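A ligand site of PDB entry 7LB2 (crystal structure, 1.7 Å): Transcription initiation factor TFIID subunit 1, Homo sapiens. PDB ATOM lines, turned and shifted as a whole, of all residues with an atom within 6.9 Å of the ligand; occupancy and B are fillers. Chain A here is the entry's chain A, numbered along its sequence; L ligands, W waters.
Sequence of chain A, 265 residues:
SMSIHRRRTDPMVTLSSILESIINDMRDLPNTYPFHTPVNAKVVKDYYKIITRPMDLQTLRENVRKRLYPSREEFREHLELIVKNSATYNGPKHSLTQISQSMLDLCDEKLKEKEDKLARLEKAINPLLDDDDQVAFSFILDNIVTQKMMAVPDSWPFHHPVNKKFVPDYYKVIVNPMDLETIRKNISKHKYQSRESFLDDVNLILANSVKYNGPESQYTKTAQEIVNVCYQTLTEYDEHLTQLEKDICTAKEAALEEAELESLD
The backbone carbonyl oxygen of Pro 161 is in hydrogen-bond range of a nitrogen (N1) of the ligand, 3.0 Å away. An oxygen (O2) of the ligand lies within hydrogen-bond range of the backbone NH of Asn 163 (2.9 Å). ND2 of Asn 213 sits at hydrogen-bond distance from O1 of the ligand (2.9 Å).
The side-chain hydroxyl (OG) of Ser 209 lies within hydrogen-bond range of the side-chain amide nitrogen (ND2) of Asn 213 (3.1 Å).
Trp 156 touches the ligand (O to C12, 3.6 Å). Pro 157 touches the ligand. Phe 158 touches the ligand (CE1 to C2, 3.8 Å). His 160 touches the ligand. CA of Val 162 touches O2 of the ligand, at 3.5 Å. Phe 166 touches the ligand. CE2 of Tyr 212 touches C3 of the ligand, 3.9 Å away. Tyr 219 touches the ligand. Hydrophobic or aromatic side chains that line the ligand: Trp 156, Pro 157, Phe 158, Val 162, Phe 166, Tyr 212 and Tyr 219.
Water W1 lies within hydrogen-bond range of OH of Tyr 170 (2.7 Å), O of Asn 208 (3.3 Å), N of Ser 209 (3.5 Å) and O1 of the ligand (3.5 Å).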
ATOM      1  N   TRP A 156      31.690   6.639  24.134  1.00  0.00           N
ATOM      2  CA  TRP A 156      30.471   6.189  24.828  1.00  0.00           C
ATOM      3  C   TRP A 156      29.199   6.968  24.522  1.00  0.00           C
ATOM      4  O   TRP A 156      28.119   6.359  24.532  1.00  0.00           O
ATOM      5  CB  TRP A 156      30.765   6.165  26.357  1.00  0.00           C
ATOM      6  CG  TRP A 156      31.066   7.569  26.924  1.00  0.00           C
ATOM      7  CD1 TRP A 156      32.298   8.099  27.073  1.00  0.00           C
ATOM      8  CD2 TRP A 156      30.145   8.574  27.390  1.00  0.00           C
ATOM      9  NE1 TRP A 156      32.228   9.383  27.562  1.00  0.00           N
ATOM     10  CE2 TRP A 156      30.901   9.700  27.742  1.00  0.00           C
ATOM     11  CE3 TRP A 156      28.749   8.652  27.503  1.00  0.00           C
ATOM     12  CZ2 TRP A 156      30.329  10.871  28.235  1.00  0.00           C
ATOM     13  CZ3 TRP A 156      28.175   9.809  27.979  1.00  0.00           C
ATOM     14  CH2 TRP A 156      28.958  10.898  28.342  1.00  0.00           C
ATOM     15  N   PRO A 157      29.228   8.291  24.282  1.00  0.00           N
ATOM     16  CA  PRO A 157      27.971   8.992  24.026  1.00  0.00           C
ATOM     17  C   PRO A 157      27.237   8.457  22.806  1.00  0.00           C
ATOM     18  O   PRO A 157      26.035   8.679  22.672  1.00  0.00           O
ATOM     19  CB  PRO A 157      28.400  10.455  23.801  1.00  0.00           C
ATOM     20  CG  PRO A 157      29.743  10.566  24.505  1.00  0.00           C
ATOM     21  CD  PRO A 157      30.384   9.202  24.211  1.00  0.00           C
ATOM     22  N   PHE A 158      27.960   7.802  21.914  1.00  0.00           N
ATOM     23  CA  PHE A 158      27.429   7.374  20.640  1.00  0.00           C
ATOM     24  C   PHE A 158      27.171   5.876  20.571  1.00  0.00           C
ATOM     25  O   PHE A 158      26.666   5.408  19.543  1.00  0.00           O
ATOM     26  CB  PHE A 158      28.381   7.828  19.515  1.00  0.00           C
ATOM     27  CG  PHE A 158      28.708   9.285  19.609  1.00  0.00           C
ATOM     28  CD1 PHE A 158      27.755  10.218  19.329  1.00  0.00           C
ATOM     29  CD2 PHE A 158      29.947   9.720  20.048  1.00  0.00           C
ATOM     30  CE1 PHE A 158      27.998  11.580  19.471  1.00  0.00           C
ATOM     31  CE2 PHE A 158      30.213  11.061  20.188  1.00  0.00           C
ATOM     32  CZ  PHE A 158      29.229  11.999  19.916  1.00  0.00           C
ATOM     33  N   HIS A 159      27.397   5.142  21.650  1.00  0.00           N
ATOM     34  CA  HIS A 159      27.208   3.703  21.629  1.00  0.00           C
ATOM     35  C   HIS A 159      25.750   3.268  21.712  1.00  0.00           C
ATOM     36  O   HIS A 159      25.454   2.123  21.368  1.00  0.00           O
ATOM     37  CB  HIS A 159      27.969   3.059  22.778  1.00  0.00           C
ATOM     38  CG  HIS A 159      29.450   3.046  22.590  1.00  0.00           C
ATOM     39  ND1 HIS A 159      30.234   2.108  23.224  1.00  0.00           N
ATOM     40  CD2 HIS A 159      30.267   3.742  21.772  1.00  0.00           C
ATOM     41  CE1 HIS A 159      31.499   2.305  22.895  1.00  0.00           C
ATOM     42  NE2 HIS A 159      31.550   3.283  21.993  1.00  0.00           N
ATOM     43  N   HIS A 160      24.863   4.089  22.265  1.00  0.00           N
ATOM     44  CA  HIS A 160      23.484   3.697  22.544  1.00  0.00           C
ATOM     45  C   HIS A 160      22.573   4.887  22.289  1.00  0.00           C
ATOM     46  O   HIS A 160      23.025   6.035  22.258  1.00  0.00           O
ATOM     47  CB  HIS A 160      23.296   3.224  23.992  1.00  0.00           C
ATOM     48  CG  HIS A 160      24.158   2.060  24.370  1.00  0.00           C
ATOM     49  ND1 HIS A 160      23.851   0.761  24.022  1.00  0.00           N
ATOM     50  CD2 HIS A 160      25.334   2.010  25.040  1.00  0.00           C
ATOM     51  CE1 HIS A 160      24.782  -0.052  24.487  1.00  0.00           C
ATOM     52  NE2 HIS A 160      25.693   0.672  25.112  1.00  0.00           N
ATOM     53  N   PRO A 161      21.280   4.656  22.112  1.00  0.00           N
ATOM     54  CA  PRO A 161      20.348   5.782  22.033  1.00  0.00           C
ATOM     55  C   PRO A 161      20.363   6.600  23.305  1.00  0.00           C
ATOM     56  O   PRO A 161      20.436   6.054  24.413  1.00  0.00           O
ATOM     57  CB  PRO A 161      18.986   5.118  21.843  1.00  0.00           C
ATOM     58  CG  PRO A 161      19.238   3.740  21.502  1.00  0.00           C
ATOM     59  CD  PRO A 161      20.588   3.369  22.032  1.00  0.00           C
ATOM     60  N   VAL A 162      20.236   7.912  23.111  1.00  0.00           N
ATOM     61  CA  VAL A 162      20.082   8.808  24.249  1.00  0.00           C
ATOM     62  C   VAL A 162      18.808   8.441  24.992  1.00  0.00           C
ATOM     63  O   VAL A 162      17.739   8.261  24.373  1.00  0.00           O
ATOM     64  CB  VAL A 162      20.045  10.260  23.779  1.00  0.00           C
ATOM     65  CG1 VAL A 162      19.646  11.165  24.910  1.00  0.00           C
ATOM     66  CG2 VAL A 162      21.369  10.666  23.235  1.00  0.00           C
ATOM     67  N   ASN A 163      18.896   8.395  26.312  1.00  0.00           N
ATOM     68  CA  ASN A 163      17.730   8.155  27.152  1.00  0.00           C
ATOM     69  C   ASN A 163      17.095   9.502  27.482  1.00  0.00           C
ATOM     70  O   ASN A 163      17.708  10.355  28.123  1.00  0.00           O
ATOM     71  CB  ASN A 163      18.143   7.414  28.430  1.00  0.00           C
ATOM     72  CG  ASN A 163      16.971   6.917  29.205  1.00  0.00           C
ATOM     73  OD1 ASN A 163      15.949   7.595  29.255  1.00  0.00           O
ATOM     74  ND2 ASN A 163      17.093   5.751  29.830  1.00  0.00           N
ATOM     75  N   LYS A 164      15.871   9.709  26.986  1.00  0.00           N
ATOM     76  CA  LYS A 164      15.186  10.981  27.166  1.00  0.00           C
ATOM     77  C   LYS A 164      14.941  11.309  28.634  1.00  0.00           C
ATOM     78  O   LYS A 164      14.807  12.494  28.997  1.00  0.00           O
ATOM     79  CB  LYS A 164      13.849  10.947  26.418  1.00  0.00           C
ATOM     80  CG  LYS A 164      13.148  12.283  26.373  1.00  0.00           C
ATOM     81  CD  LYS A 164      12.090  12.398  25.241  1.00  0.00           C
ATOM     82  CE  LYS A 164      10.943  11.526  25.508  1.00  0.00           C
ATOM     83  NZ  LYS A 164       9.927  11.669  24.415  1.00  0.00           N
ATOM     84  N   PHE A 166      17.117  11.175  30.821  1.00  0.00           N
ATOM     85  CA  PHE A 166      18.299  11.855  31.298  1.00  0.00           C
ATOM     86  C   PHE A 166      18.623  13.116  30.513  1.00  0.00           C
ATOM     87  O   PHE A 166      19.214  14.055  31.065  1.00  0.00           O
ATOM     88  CB  PHE A 166      19.531  10.963  31.165  1.00  0.00           C
ATOM     89  CG  PHE A 166      19.446   9.642  31.854  1.00  0.00           C
ATOM     90  CD1 PHE A 166      18.830   9.515  33.062  1.00  0.00           C
ATOM     91  CD2 PHE A 166      20.092   8.560  31.300  1.00  0.00           C
ATOM     92  CE1 PHE A 166      18.797   8.298  33.702  1.00  0.00           C
ATOM     93  CE2 PHE A 166      20.080   7.342  31.947  1.00  0.00           C
ATOM     94  CZ  PHE A 166      19.429   7.224  33.132  1.00  0.00           C
ATOM     95  N   VAL A 167      18.176  13.190  29.273  1.00  0.00           N
ATOM     96  CA  VAL A 167      18.381  14.363  28.424  1.00  0.00           C
ATOM     97  C   VAL A 167      17.040  14.749  27.820  1.00  0.00           C
ATOM     98  O   VAL A 167      16.728  14.336  26.682  1.00  0.00           O
ATOM     99  CB  VAL A 167      19.400  14.055  27.316  1.00  0.00           C
ATOM    100  CG1 VAL A 167      19.815  15.332  26.624  1.00  0.00           C
ATOM    101  CG2 VAL A 167      20.621  13.307  27.893  1.00  0.00           C
ATOM    102  N   TYR A 170      16.400  16.078  24.069  1.00  0.00           N
ATOM    103  CA  TYR A 170      17.266  15.579  23.011  1.00  0.00           C
ATOM    104  C   TYR A 170      16.477  15.331  21.724  1.00  0.00           C
ATOM    105  O   TYR A 170      16.922  15.725  20.630  1.00  0.00           O
ATOM    106  CB  TYR A 170      17.976  14.293  23.437  1.00  0.00           C
ATOM    107  CG  TYR A 170      18.970  13.855  22.407  1.00  0.00           C
ATOM    108  CD1 TYR A 170      20.184  14.503  22.291  1.00  0.00           C
ATOM    109  CD2 TYR A 170      18.669  12.842  21.498  1.00  0.00           C
ATOM    110  CE1 TYR A 170      21.103  14.138  21.309  1.00  0.00           C
ATOM    111  CE2 TYR A 170      19.568  12.460  20.501  1.00  0.00           C
ATOM    112  CZ  TYR A 170      20.773  13.143  20.426  1.00  0.00           C
ATOM    113  OH  TYR A 170      21.694  12.797  19.475  1.00  0.00           O
ATOM    114  N   ASP A 179      22.671   5.820  16.475  1.00  0.00           N
ATOM    115  CA  ASP A 179      23.716   5.476  17.433  1.00  0.00           C
ATOM    116  C   ASP A 179      24.291   4.148  16.966  1.00  0.00           C
ATOM    117  O   ASP A 179      23.712   3.469  16.110  1.00  0.00           O
ATOM    118  CB  ASP A 179      23.132   5.350  18.827  1.00  0.00           C
ATOM    119  CG  ASP A 179      22.179   4.266  18.890  1.00  0.00           C
ATOM    120  OD1 ASP A 179      20.992   4.534  18.595  1.00  0.00           O
ATOM    121  OD2 ASP A 179      22.598   3.123  19.235  1.00  0.00           O
ATOM    122  N   ASN A 208      24.017  14.574  13.869  1.00  0.00           N
ATOM    123  CA  ASN A 208      23.278  14.869  15.087  1.00  0.00           C
ATOM    124  C   ASN A 208      24.132  15.508  16.154  1.00  0.00           C
ATOM    125  O   ASN A 208      23.640  16.362  16.897  1.00  0.00           O
ATOM    126  CB  ASN A 208      22.652  13.578  15.620  1.00  0.00           C
ATOM    127  CG  ASN A 208      21.546  13.080  14.710  1.00  0.00           C
ATOM    128  OD1 ASN A 208      20.980  13.841  13.941  1.00  0.00           O
ATOM    129  ND2 ASN A 208      21.211  11.817  14.834  1.00  0.00           N
ATOM    130  N   SER A 209      25.417  15.138  16.237  1.00  0.00           N
ATOM    131  CA  SER A 209      26.301  15.771  17.206  1.00  0.00           C
ATOM    132  C   SER A 209      26.552  17.224  16.841  1.00  0.00           C
ATOM    133  O   SER A 209      26.590  18.105  17.713  1.00  0.00           O
ATOM    134  CB  SER A 209      27.596  14.979  17.356  1.00  0.00           C
ATOM    135  OG  SER A 209      28.374  15.572  18.415  1.00  0.00           O
ATOM    136  N   TYR A 212      23.243  19.033  17.857  1.00  0.00           N
ATOM    137  CA  TYR A 212      22.899  19.131  19.280  1.00  0.00           C
ATOM    138  C   TYR A 212      24.027  19.766  20.093  1.00  0.00           C
ATOM    139  O   TYR A 212      23.784  20.612  20.955  1.00  0.00           O
ATOM    140  CB  TYR A 212      22.545  17.707  19.824  1.00  0.00           C
ATOM    141  CG  TYR A 212      21.976  17.799  21.229  1.00  0.00           C
ATOM    142  CD1 TYR A 212      20.636  18.146  21.414  1.00  0.00           C
ATOM    143  CD2 TYR A 212      22.775  17.638  22.352  1.00  0.00           C
ATOM    144  CE1 TYR A 212      20.111  18.306  22.664  1.00  0.00           C
ATOM    145  CE2 TYR A 212      22.243  17.788  23.621  1.00  0.00           C
ATOM    146  CZ  TYR A 212      20.921  18.127  23.777  1.00  0.00           C
ATOM    147  OH  TYR A 212      20.395  18.296  25.031  1.00  0.00           O
ATOM    148  N   ASN A 213      25.283  19.413  19.796  1.00  0.00           N
ATOM    149  CA  ASN A 213      26.444  19.840  20.583  1.00  0.00           C
ATOM    150  C   ASN A 213      27.231  20.989  19.976  1.00  0.00           C
ATOM    151  O   ASN A 213      27.977  21.665  20.699  1.00  0.00           O
ATOM    152  CB  ASN A 213      27.360  18.635  20.775  1.00  0.00           C
ATOM    153  CG  ASN A 213      26.645  17.505  21.491  1.00  0.00           C
ATOM    154  OD1 ASN A 213      26.091  17.710  22.554  1.00  0.00           O
ATOM    155  ND2 ASN A 213      26.615  16.329  20.882  1.00  0.00           N
ATOM    156  N   TYR A 219      32.306  16.444  21.858  1.00  0.00           N
ATOM    157  CA  TYR A 219      31.437  15.371  21.384  1.00  0.00           C
ATOM    158  C   TYR A 219      31.512  15.221  19.873  1.00  0.00           C
ATOM    159  O   TYR A 219      31.639  14.101  19.352  1.00  0.00           O
ATOM    160  CB  TYR A 219      29.985  15.656  21.751  1.00  0.00           C
ATOM    161  CG  TYR A 219      29.651  15.548  23.209  1.00  0.00           C
ATOM    162  CD1 TYR A 219      29.698  14.324  23.830  1.00  0.00           C
ATOM    163  CD2 TYR A 219      29.240  16.642  23.950  1.00  0.00           C
ATOM    164  CE1 TYR A 219      29.362  14.188  25.163  1.00  0.00           C
ATOM    165  CE2 TYR A 219      28.892  16.519  25.279  1.00  0.00           C
ATOM    166  CZ  TYR A 219      28.958  15.283  25.881  1.00  0.00           C
ATOM    167  OH  TYR A 219      28.621  15.142  27.200  1.00  0.00           O
HETATM  168  C1  LIG L   1      24.996  13.874  24.769  1.00  0.00           C
HETATM  169  C2  LIG L   1      25.717  12.914  22.240  1.00  0.00           C
HETATM  170  C3  LIG L   1      23.516  14.297  24.804  1.00  0.00           C
HETATM  171  C4  LIG L   1      24.577  11.173  27.928  1.00  0.00           C
HETATM  172  C5  LIG L   1      23.169  11.284  31.515  1.00  0.00           C
HETATM  173  C6  LIG L   1      23.946  12.310  32.096  1.00  0.00           C
HETATM  174  C7  LIG L   1      24.929  12.973  31.278  1.00  0.00           C
HETATM  175  C8  LIG L   1      26.151  13.282  29.158  1.00  0.00           C
HETATM  176  C9  LIG L   1      26.678  14.693  31.067  1.00  0.00           C
HETATM  177  C10 LIG L   1      23.912   7.935  26.343  1.00  0.00           C
HETATM  178  C11 LIG L   1      23.972   7.019  25.167  1.00  0.00           C
HETATM  179  C12 LIG L   1      25.003   6.864  26.285  1.00  0.00           C
HETATM  180  C13 LIG L   1      24.249   9.412  26.534  1.00  0.00           C
HETATM  181  C14 LIG L   1      24.508  10.216  25.421  1.00  0.00           C
HETATM  182  C15 LIG L   1      24.781  11.560  25.695  1.00  0.00           C
HETATM  183  C16 LIG L   1      25.774  14.649  23.716  1.00  0.00           C
HETATM  184  C17 LIG L   1      24.904  11.989  23.184  1.00  0.00           C
HETATM  185  C18 LIG L   1      24.433  11.594  29.400  1.00  0.00           C
HETATM  186  C19 LIG L   1      23.442  10.948  30.183  1.00  0.00           C
HETATM  187  C20 LIG L   1      25.162  12.641  29.955  1.00  0.00           C
HETATM  188  C21 LIG L   1      26.900  14.300  29.752  1.00  0.00           C
HETATM  189  C22 LIG L   1      25.706  14.040  31.822  1.00  0.00           C
HETATM  190  C23 LIG L   1      23.436   7.214  28.904  1.00  0.00           C
HETATM  191  N1  LIG L   1      21.908   6.160  27.067  1.00  0.00           N
HETATM  192  N2  LIG L   1      25.062  12.416  24.569  1.00  0.00           N
HETATM  193  N3  LIG L   1      24.792  12.040  26.931  1.00  0.00           N
HETATM  194  N4  LIG L   1      24.285   9.917  27.744  1.00  0.00           N
HETATM  195  O1  LIG L   1      25.422  14.257  22.438  1.00  0.00           O
HETATM  196  O2  LIG L   1      21.512   8.701  27.494  1.00  0.00           O
HETATM  197  S1  LIG L   1      22.422   7.540  27.437  1.00  0.00           S
HETATM  198  O   HOH W   1      24.098  14.030  19.229  1.00  0.00           O
